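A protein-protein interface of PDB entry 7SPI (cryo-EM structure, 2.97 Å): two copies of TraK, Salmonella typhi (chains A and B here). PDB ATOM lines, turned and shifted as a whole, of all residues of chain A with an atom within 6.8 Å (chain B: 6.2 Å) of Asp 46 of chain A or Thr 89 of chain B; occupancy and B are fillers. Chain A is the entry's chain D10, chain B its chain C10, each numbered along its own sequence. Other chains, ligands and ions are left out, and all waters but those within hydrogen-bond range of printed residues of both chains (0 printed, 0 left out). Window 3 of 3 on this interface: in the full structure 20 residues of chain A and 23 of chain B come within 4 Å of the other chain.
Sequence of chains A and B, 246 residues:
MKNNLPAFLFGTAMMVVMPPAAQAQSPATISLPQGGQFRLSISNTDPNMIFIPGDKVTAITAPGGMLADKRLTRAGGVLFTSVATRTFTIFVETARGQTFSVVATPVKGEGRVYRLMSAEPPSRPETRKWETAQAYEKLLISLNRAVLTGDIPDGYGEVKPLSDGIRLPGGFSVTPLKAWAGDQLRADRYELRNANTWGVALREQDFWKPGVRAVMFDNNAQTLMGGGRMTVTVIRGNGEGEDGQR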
ATOM      1  N   ILE A  42      11.314 -13.710  30.207  1.00  0.00           N
ATOM      2  CA  ILE A  42       9.886 -13.408  30.099  1.00  0.00           C
ATOM      3  C   ILE A  42       9.721 -12.364  28.999  1.00  0.00           C
ATOM      4  O   ILE A  42      10.663 -12.115  28.249  1.00  0.00           O
ATOM      5  CB  ILE A  42       9.298 -12.873  31.416  1.00  0.00           C
ATOM      6  CG1 ILE A  42      10.101 -11.672  31.913  1.00  0.00           C
ATOM      7  CG2 ILE A  42       9.266 -13.967  32.471  1.00  0.00           C
ATOM      8  CD1 ILE A  42       9.419 -10.927  33.033  1.00  0.00           C
ATOM      9  N   SER A  43       8.547 -11.746  28.899  1.00  0.00           N
ATOM     10  CA  SER A  43       8.376 -10.688  27.905  1.00  0.00           C
ATOM     11  C   SER A  43       7.904  -9.350  28.439  1.00  0.00           C
ATOM     12  O   SER A  43       6.987  -9.290  29.261  1.00  0.00           O
ATOM     13  CB  SER A  43       7.413 -11.152  26.809  1.00  0.00           C
ATOM     14  OG  SER A  43       6.953 -10.053  26.043  1.00  0.00           O
ATOM     15  N   ASN A  44       8.525  -8.273  27.976  1.00  0.00           N
ATOM     16  CA  ASN A  44       8.093  -6.927  28.362  1.00  0.00           C
ATOM     17  C   ASN A  44       6.783  -6.507  27.709  1.00  0.00           C
ATOM     18  O   ASN A  44       5.912  -5.944  28.367  1.00  0.00           O
ATOM     19  CB  ASN A  44       9.197  -5.917  28.044  1.00  0.00           C
ATOM     20  CG  ASN A  44      10.128  -6.397  26.951  1.00  0.00           C
ATOM     21  OD1 ASN A  44       9.697  -6.974  25.957  1.00  0.00           O
ATOM     22  ND2 ASN A  44      11.416  -6.144  27.126  1.00  0.00           N
ATOM     23  N   THR A  45       6.644  -6.755  26.415  1.00  0.00           N
ATOM     24  CA  THR A  45       5.412  -6.439  25.693  1.00  0.00           C
ATOM     25  C   THR A  45       4.122  -7.183  26.035  1.00  0.00           C
ATOM     26  O   THR A  45       3.064  -6.562  26.086  1.00  0.00           O
ATOM     27  CB  THR A  45       5.635  -6.595  24.187  1.00  0.00           C
ATOM     28  OG1 THR A  45       6.594  -7.632  23.957  1.00  0.00           O
ATOM     29  CG2 THR A  45       6.170  -5.309  23.601  1.00  0.00           C
ATOM     30  N   ASP A  46       4.181  -8.488  26.288  1.00  0.00           N
ATOM     31  CA  ASP A  46       2.941  -9.261  26.467  1.00  0.00           C
ATOM     32  C   ASP A  46       2.818 -10.008  27.775  1.00  0.00           C
ATOM     33  O   ASP A  46       3.817 -10.271  28.417  1.00  0.00           O
ATOM     34  CB  ASP A  46       2.799 -10.249  25.309  1.00  0.00           C
ATOM     35  CG  ASP A  46       2.454  -9.573  23.999  1.00  0.00           C
ATOM     36  OD1 ASP A  46       1.640  -8.629  24.014  1.00  0.00           O
ATOM     37  OD2 ASP A  46       2.984  -9.996  22.952  1.00  0.00           O
ATOM     38  N   PRO A  47       1.585 -10.347  28.182  1.00  0.00           N
ATOM     39  CA  PRO A  47       1.392 -11.010  29.471  1.00  0.00           C
ATOM     40  C   PRO A  47       2.061 -12.367  29.530  1.00  0.00           C
ATOM     41  O   PRO A  47       2.171 -13.026  28.504  1.00  0.00           O
ATOM     42  CB  PRO A  47      -0.121 -11.151  29.574  1.00  0.00           C
ATOM     43  CG  PRO A  47      -0.663 -10.075  28.707  1.00  0.00           C
ATOM     44  CD  PRO A  47       0.303  -9.959  27.571  1.00  0.00           C
ATOM     45  N   ASN A  48       2.528 -12.777  30.706  1.00  0.00           N
ATOM     46  CA  ASN A  48       3.257 -14.028  30.836  1.00  0.00           C
ATOM     47  C   ASN A  48       2.567 -14.846  31.906  1.00  0.00           C
ATOM     48  O   ASN A  48       1.929 -14.293  32.788  1.00  0.00           O
ATOM     49  CB  ASN A  48       4.705 -13.762  31.221  1.00  0.00           C
ATOM     50  CG  ASN A  48       5.407 -12.822  30.276  1.00  0.00           C
ATOM     51  OD1 ASN A  48       5.887 -13.229  29.225  1.00  0.00           O
ATOM     52  ND2 ASN A  48       5.492 -11.557  30.659  1.00  0.00           N
ATOM     53  N   PHE A  80       1.169 -12.183  34.595  1.00  0.00           N
ATOM     54  CA  PHE A  80       1.971 -11.031  34.976  1.00  0.00           C
ATOM     55  C   PHE A  80       2.613 -10.301  33.807  1.00  0.00           C
ATOM     56  O   PHE A  80       3.018 -10.917  32.829  1.00  0.00           O
ATOM     57  CB  PHE A  80       3.024 -11.418  36.026  1.00  0.00           C
ATOM     58  CG  PHE A  80       4.007 -12.456  35.571  1.00  0.00           C
ATOM     59  CD1 PHE A  80       3.747 -13.796  35.758  1.00  0.00           C
ATOM     60  CD2 PHE A  80       5.209 -12.085  34.997  1.00  0.00           C
ATOM     61  CE1 PHE A  80       4.650 -14.749  35.348  1.00  0.00           C
ATOM     62  CE2 PHE A  80       6.119 -13.034  34.587  1.00  0.00           C
ATOM     63  CZ  PHE A  80       5.839 -14.371  34.763  1.00  0.00           C
ATOM     64  N   THR A  81       2.713  -8.983  33.907  1.00  0.00           N
ATOM     65  CA  THR A  81       3.297  -8.180  32.842  1.00  0.00           C
ATOM     66  C   THR A  81       4.435  -7.361  33.409  1.00  0.00           C
ATOM     67  O   THR A  81       4.333  -6.864  34.515  1.00  0.00           O
ATOM     68  CB  THR A  81       2.263  -7.198  32.285  1.00  0.00           C
ATOM     69  OG1 THR A  81       1.582  -6.564  33.373  1.00  0.00           O
ATOM     70  CG2 THR A  81       1.243  -7.904  31.426  1.00  0.00           C
ATOM     71  N   SER A  82       5.522  -7.226  32.667  1.00  0.00           N
ATOM     72  CA  SER A  82       6.645  -6.421  33.128  1.00  0.00           C
ATOM     73  C   SER A  82       7.057  -5.301  32.191  1.00  0.00           C
ATOM     74  O   SER A  82       7.239  -5.523  31.011  1.00  0.00           O
ATOM     75  CB  SER A  82       7.863  -7.301  33.363  1.00  0.00           C
ATOM     76  OG  SER A  82       8.441  -7.713  32.139  1.00  0.00           O
ATOM     77  N   VAL A 107      12.514  -9.703  27.701  1.00  0.00           N
ATOM     78  CA  VAL A 107      12.936  -9.594  26.307  1.00  0.00           C
ATOM     79  C   VAL A 107      11.723  -9.445  25.393  1.00  0.00           C
ATOM     80  O   VAL A 107      10.627  -9.858  25.748  1.00  0.00           O
ATOM     81  CB  VAL A 107      13.782 -10.816  25.905  1.00  0.00           C
ATOM     82  CG1 VAL A 107      12.941 -12.081  25.858  1.00  0.00           C
ATOM     83  CG2 VAL A 107      14.517 -10.587  24.595  1.00  0.00           C
ATOM     84  N   GLY A 109       8.962 -10.086  22.646  1.00  0.00           N
ATOM     85  CA  GLY A 109       8.392 -11.283  22.063  1.00  0.00           C
ATOM     86  C   GLY A 109       7.031 -11.685  22.568  1.00  0.00           C
ATOM     87  O   GLY A 109       6.354 -10.909  23.233  1.00  0.00           O
ATOM     88  N   GLU A 110       6.620 -12.901  22.240  1.00  0.00           N
ATOM     89  CA  GLU A 110       5.341 -13.410  22.698  1.00  0.00           C
ATOM     90  C   GLU A 110       5.350 -13.729  24.180  1.00  0.00           C
ATOM     91  O   GLU A 110       6.386 -14.053  24.739  1.00  0.00           O
ATOM     92  CB  GLU A 110       4.974 -14.650  21.887  1.00  0.00           C
ATOM     93  CG  GLU A 110       6.152 -15.556  21.562  1.00  0.00           C
ATOM     94  CD  GLU A 110       6.189 -16.814  22.409  1.00  0.00           C
ATOM     95  OE1 GLU A 110       7.276 -17.420  22.531  1.00  0.00           O
ATOM     96  OE2 GLU A 110       5.135 -17.200  22.954  1.00  0.00           O
ATOM     97  N   GLY A 111       4.196 -13.649  24.819  1.00  0.00           N
ATOM     98  CA  GLY A 111       4.108 -13.978  26.220  1.00  0.00           C
ATOM     99  C   GLY A 111       4.491 -15.414  26.402  1.00  0.00           C
ATOM    100  O   GLY A 111       4.043 -16.271  25.650  1.00  0.00           O
ATOM    101  N   ARG A 112       5.346 -15.694  27.384  1.00  0.00           N
ATOM    102  CA  ARG A 112       5.847 -17.043  27.595  1.00  0.00           C
ATOM    103  C   ARG A 112       5.162 -17.710  28.749  1.00  0.00           C
ATOM    104  O   ARG A 112       4.907 -17.075  29.762  1.00  0.00           O
ATOM    105  CB  ARG A 112       7.354 -16.998  27.774  1.00  0.00           C
ATOM    106  CG  ARG A 112       8.080 -16.652  26.491  1.00  0.00           C
ATOM    107  CD  ARG A 112       9.459 -16.083  26.750  1.00  0.00           C
ATOM    108  NE  ARG A 112      10.149 -15.764  25.507  1.00  0.00           N
ATOM    109  CZ  ARG A 112      10.092 -14.584  24.900  1.00  0.00           C
ATOM    110  NH1 ARG A 112       9.379 -13.599  25.424  1.00  0.00           N
ATOM    111  NH2 ARG A 112      10.752 -14.387  23.770  1.00  0.00           N
ATOM    112  N   GLN B  37       0.534 -22.311  22.569  1.00  0.00           N
ATOM    113  CA  GLN B  37       0.869 -21.006  22.026  1.00  0.00           C
ATOM    114  C   GLN B  37       0.677 -21.130  20.530  1.00  0.00           C
ATOM    115  O   GLN B  37       1.553 -21.633  19.826  1.00  0.00           O
ATOM    116  CB  GLN B  37       2.315 -20.639  22.344  1.00  0.00           C
ATOM    117  CG  GLN B  37       2.670 -19.188  22.067  1.00  0.00           C
ATOM    118  CD  GLN B  37       2.313 -18.275  23.221  1.00  0.00           C
ATOM    119  OE1 GLN B  37       1.420 -17.437  23.115  1.00  0.00           O
ATOM    120  NE2 GLN B  37       3.003 -18.444  24.342  1.00  0.00           N
ATOM    121  N   THR B  61      -7.939 -12.199  28.171  1.00  0.00           N
ATOM    122  CA  THR B  61      -7.059 -11.146  28.627  1.00  0.00           C
ATOM    123  C   THR B  61      -6.042 -10.807  27.595  1.00  0.00           C
ATOM    124  O   THR B  61      -5.298 -11.657  27.153  1.00  0.00           O
ATOM    125  CB  THR B  61      -6.294 -11.558  29.888  1.00  0.00           C
ATOM    126  OG1 THR B  61      -7.219 -12.017  30.881  1.00  0.00           O
ATOM    127  CG2 THR B  61      -5.498 -10.394  30.453  1.00  0.00           C
ATOM    128  N   ALA B  62      -5.957  -9.541  27.248  1.00  0.00           N
ATOM    129  CA  ALA B  62      -4.963  -9.126  26.320  1.00  0.00           C
ATOM    130  C   ALA B  62      -4.240  -7.888  26.876  1.00  0.00           C
ATOM    131  O   ALA B  62      -4.651  -7.390  27.916  1.00  0.00           O
ATOM    132  CB  ALA B  62      -5.594  -8.822  24.988  1.00  0.00           C
ATOM    133  N   PRO B  63      -3.165  -7.379  26.213  1.00  0.00           N
ATOM    134  CA  PRO B  63      -2.491  -6.152  26.649  1.00  0.00           C
ATOM    135  C   PRO B  63      -3.447  -4.967  26.623  1.00  0.00           C
ATOM    136  O   PRO B  63      -4.344  -4.890  25.782  1.00  0.00           O
ATOM    137  CB  PRO B  63      -1.360  -5.988  25.631  1.00  0.00           C
ATOM    138  CG  PRO B  63      -1.083  -7.366  25.164  1.00  0.00           C
ATOM    139  CD  PRO B  63      -2.396  -8.093  25.180  1.00  0.00           C
ATOM    140  N   ARG B  86      -0.352  -4.321  15.752  1.00  0.00           N
ATOM    141  CA  ARG B  86       0.770  -5.169  16.172  1.00  0.00           C
ATOM    142  C   ARG B  86       0.399  -6.565  16.601  1.00  0.00           C
ATOM    143  O   ARG B  86      -0.689  -6.790  17.114  1.00  0.00           O
ATOM    144  CB  ARG B  86       1.573  -4.508  17.284  1.00  0.00           C
ATOM    145  CG  ARG B  86       0.913  -4.505  18.650  1.00  0.00           C
ATOM    146  CD  ARG B  86       1.928  -4.160  19.723  1.00  0.00           C
ATOM    147  NE  ARG B  86       1.384  -4.289  21.069  1.00  0.00           N
ATOM    148  CZ  ARG B  86       1.511  -5.372  21.825  1.00  0.00           C
ATOM    149  NH1 ARG B  86       2.169  -6.428  21.372  1.00  0.00           N
ATOM    150  NH2 ARG B  86       0.982  -5.397  23.039  1.00  0.00           N
ATOM    151  N   THR B  87       1.295  -7.513  16.396  1.00  0.00           N
ATOM    152  CA  THR B  87       1.064  -8.860  16.868  1.00  0.00           C
ATOM    153  C   THR B  87       1.014  -8.885  18.382  1.00  0.00           C
ATOM    154  O   THR B  87       1.861  -8.294  19.031  1.00  0.00           O
ATOM    155  CB  THR B  87       2.200  -9.746  16.387  1.00  0.00           C
ATOM    156  OG1 THR B  87       2.258  -9.714  14.958  1.00  0.00           O
ATOM    157  CG2 THR B  87       2.035 -11.158  16.854  1.00  0.00           C
ATOM    158  N   PHE B  88       0.051  -9.582  18.962  1.00  0.00           N
ATOM    159  CA  PHE B  88      -0.093  -9.605  20.400  1.00  0.00           C
ATOM    160  C   PHE B  88      -0.448 -10.955  20.973  1.00  0.00           C
ATOM    161  O   PHE B  88      -1.153 -11.707  20.341  1.00  0.00           O
ATOM    162  CB  PHE B  88      -1.063  -8.536  20.883  1.00  0.00           C
ATOM    163  CG  PHE B  88      -2.460  -8.647  20.350  1.00  0.00           C
ATOM    164  CD1 PHE B  88      -2.786  -8.155  19.102  1.00  0.00           C
ATOM    165  CD2 PHE B  88      -3.468  -9.157  21.144  1.00  0.00           C
ATOM    166  CE1 PHE B  88      -4.078  -8.224  18.631  1.00  0.00           C
ATOM    167  CE2 PHE B  88      -4.759  -9.230  20.681  1.00  0.00           C
ATOM    168  CZ  PHE B  88      -5.067  -8.761  19.423  1.00  0.00           C
ATOM    169  N   THR B  89      -0.216 -11.191  22.247  1.00  0.00           N
ATOM    170  CA  THR B  89      -0.671 -12.443  22.841  1.00  0.00           C
ATOM    171  C   THR B  89      -1.937 -12.282  23.643  1.00  0.00           C
ATOM    172  O   THR B  89      -2.046 -11.366  24.429  1.00  0.00           O
ATOM    173  CB  THR B  89       0.418 -13.115  23.706  1.00  0.00           C
ATOM    174  OG1 THR B  89       1.583 -13.340  22.907  1.00  0.00           O
ATOM    175  CG2 THR B  89      -0.051 -14.438  24.260  1.00  0.00           C
ATOM    176  N   ILE B  90      -2.910 -13.164  23.437  1.00  0.00           N
ATOM    177  CA  ILE B  90      -4.138 -13.147  24.230  1.00  0.00           C
ATOM    178  C   ILE B  90      -4.309 -14.445  24.999  1.00  0.00           C
ATOM    179  O   ILE B  90      -3.874 -15.475  24.546  1.00  0.00           O
ATOM    180  CB  ILE B  90      -5.354 -12.781  23.354  1.00  0.00           C
ATOM    181  CG1 ILE B  90      -6.504 -13.762  23.489  1.00  0.00           C
ATOM    182  CG2 ILE B  90      -4.953 -12.698  21.890  1.00  0.00           C
ATOM    183  CD1 ILE B  90      -7.494 -13.608  22.359  1.00  0.00           C
ATOM    184  N   PHE B  91      -4.868 -14.384  26.196  1.00  0.00           N
ATOM    185  CA  PHE B  91      -5.038 -15.565  27.037  1.00  0.00           C
ATOM    186  C   PHE B  91      -6.471 -15.865  27.336  1.00  0.00           C
ATOM    187  O   PHE B  91      -7.182 -15.010  27.809  1.00  0.00           O
ATOM    188  CB  PHE B  91      -4.364 -15.370  28.385  1.00  0.00           C
ATOM    189  CG  PHE B  91      -2.871 -15.516  28.348  1.00  0.00           C
ATOM    190  CD1 PHE B  91      -2.067 -14.458  27.975  1.00  0.00           C
ATOM    191  CD2 PHE B  91      -2.274 -16.709  28.696  1.00  0.00           C
ATOM    192  CE1 PHE B  91      -0.699 -14.589  27.934  1.00  0.00           C
ATOM    193  CE2 PHE B  91      -0.901 -16.845  28.662  1.00  0.00           C
ATOM    194  CZ  PHE B  91      -0.112 -15.785  28.279  1.00  0.00           C
ATOM    195  N   SER B 101      -3.209 -19.897  25.215  1.00  0.00           N
ATOM    196  CA  SER B 101      -2.637 -18.645  24.744  1.00  0.00           C
ATOM    197  C   SER B 101      -2.512 -18.671  23.228  1.00  0.00           C
ATOM    198  O   SER B 101      -2.081 -19.673  22.647  1.00  0.00           O
ATOM    199  CB  SER B 101      -1.270 -18.399  25.384  1.00  0.00           C
ATOM    200  OG  SER B 101      -0.257 -19.108  24.699  1.00  0.00           O
ATOM    201  N   VAL B 102      -2.958 -17.596  22.596  1.00  0.00           N
ATOM    202  CA  VAL B 102      -2.825 -17.469  21.163  1.00  0.00           C
ATOM    203  C   VAL B 102      -2.148 -16.157  20.886  1.00  0.00           C
ATOM    204  O   VAL B 102      -2.374 -15.191  21.577  1.00  0.00           O
ATOM    205  CB  VAL B 102      -4.194 -17.529  20.471  1.00  0.00           C
ATOM    206  CG1 VAL B 102      -4.792 -18.921  20.597  1.00  0.00           C
ATOM    207  CG2 VAL B 102      -5.150 -16.499  21.046  1.00  0.00           C
ATOM    208  N   VAL B 103      -1.279 -16.126  19.900  1.00  0.00           N
ATOM    209  CA  VAL B 103      -0.646 -14.894  19.514  1.00  0.00           C
ATOM    210  C   VAL B 103      -1.396 -14.460  18.289  1.00  0.00           C
ATOM    211  O   VAL B 103      -1.335 -15.126  17.272  1.00  0.00           O
ATOM    212  CB  VAL B 103       0.815 -15.109  19.159  1.00  0.00           C
ATOM    213  CG1 VAL B 103       1.555 -13.792  19.157  1.00  0.00           C
ATOM    214  CG2 VAL B 103       1.459 -16.055  20.142  1.00  0.00           C
ATOM    215  N   ALA B 104      -2.069 -13.320  18.352  1.00  0.00           N
ATOM    216  CA  ALA B 104      -2.907 -12.876  17.271  1.00  0.00           C
ATOM    217  C   ALA B 104      -2.352 -11.706  16.516  1.00  0.00           C
ATOM    218  O   ALA B 104      -2.243 -10.638  17.063  1.00  0.00           O
ATOM    219  CB  ALA B 104      -4.205 -12.467  17.890  1.00  0.00           C
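Of the printed residues of chain B, Asp 46 of chain A touches Pro 63 (3.2 Å), Arg 86 (3.4 Å) and Thr 89 (3.5 Å). Printed residues of chain A within 4 Å of Thr 89 of chain B: Asp 46, Glu 110 and Gly 111. Printed residues of chain A within 4 Å of Phe 91 of chain B: Pro 47. Printed residues of chain B within 4 Å of Gly 111 of chain A: Gln 37 and Thr 89. Printed residues of chain B within 4 Å of Pro 47 of chain A: Pro 63 (3.8 Å) and Phe 91 (3.3 Å). Of the printed residues of chain B, Glu 110 of chain A touches Gln 37 (2.8 Å) and Thr 89 (3.8 Å). Asn 44 of chain A touches none of the printed residues of chain B. The nearest printed residue of chain B that does not touch Asp 46 of chain A is Phe 88 of chain B (4.02 Å). The nearest residue of chain A that does not touch Thr 89 of chain B is Pro 47 of chain A (4.2 Å). The nearest printed residue of chain B that does not touch Pro 47 of chain A is Thr 89 of chain B (4.2 Å).
OE1 of Gln 37 of chain B sits at hydrogen-bond distance from OG of Ser 101 of chain B. OG of Ser 43 of chain A is in hydrogen-bond range of OG1 of Thr 45 of chain A (3.2 Å). The side-chain hydroxyl (OG) of Ser 43 of chain A is in hydrogen-bond range of the backbone NH (N) of Asp 46 of chain A (3.2 Å). The side-chain hydroxyl of Thr 45 of chain A is in hydrogen-bond range of the backbone carbonyl oxygen of Gly 109 of chain A, 3.4 Å away. The side-chain amide nitrogen (ND2) of Asn 48 of chain A lies within hydrogen-bond range of the backbone carbonyl oxygen (O) of Asp 46 of chain A (3.1 Å). The backbone carbonyl oxygen of Glu 110 of chain A lies within hydrogen-bond range of the guanidinium group of Arg 112 of chain A, 3.1 Å away.
NE2 of Gln 37 of chain B lies within hydrogen-bond range of OE2 of Glu 110 of chain A (2.8 Å). NE2 of Gln 37 of chain B lies within hydrogen-bond range of O of Gly 111 of chain A (2.7 Å). NH2 of Arg 86 of chain B is in salt-bridge range of OD1 of Asp 46 of chain A, 3.4 Å away. N of Thr 89 of chain B is in hydrogen-bond range of OD2 of Asp 46 of chain A (3.5 Å). OG1 of Thr 89 of chain B lies within hydrogen-bond range of N of Gly 111 of chain A (3.3 Å).
No position is printed for both chains.
Of the 15 printed residues of chain A, 5 touch a printed residue of chain B. Printed residues of chain A that touch a printed residue of chain B: Thr 45, Asp 46, Pro 47, Glu 110 and Gly 111. Hydrophobic or aromatic side chains of chain A that line the printed part of chain B: Pro 47. Among the printed residues, Asp or Glu carboxylates within 4 Å of a Lys or Arg side-chain nitrogen of the other chain: Asp 46 of chain A with Arg 86 of chain B (3.4 Å).
NH2 of Arg 86 of chain B touches O of Thr 45 of chain A (3.9 Å). Pro 63 of chain B touches Asp 46 of chain A (CG to OD1, 3.2 Å). Pro 47 of chain A touches Pro 63 of chain B. Pro 47 of chain A touches Phe 91 of chain B (O to CE1, 3.3 Å). Glu 110 of chain A touches Thr 89 of chain B (CA to OG1, 3.8 Å).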
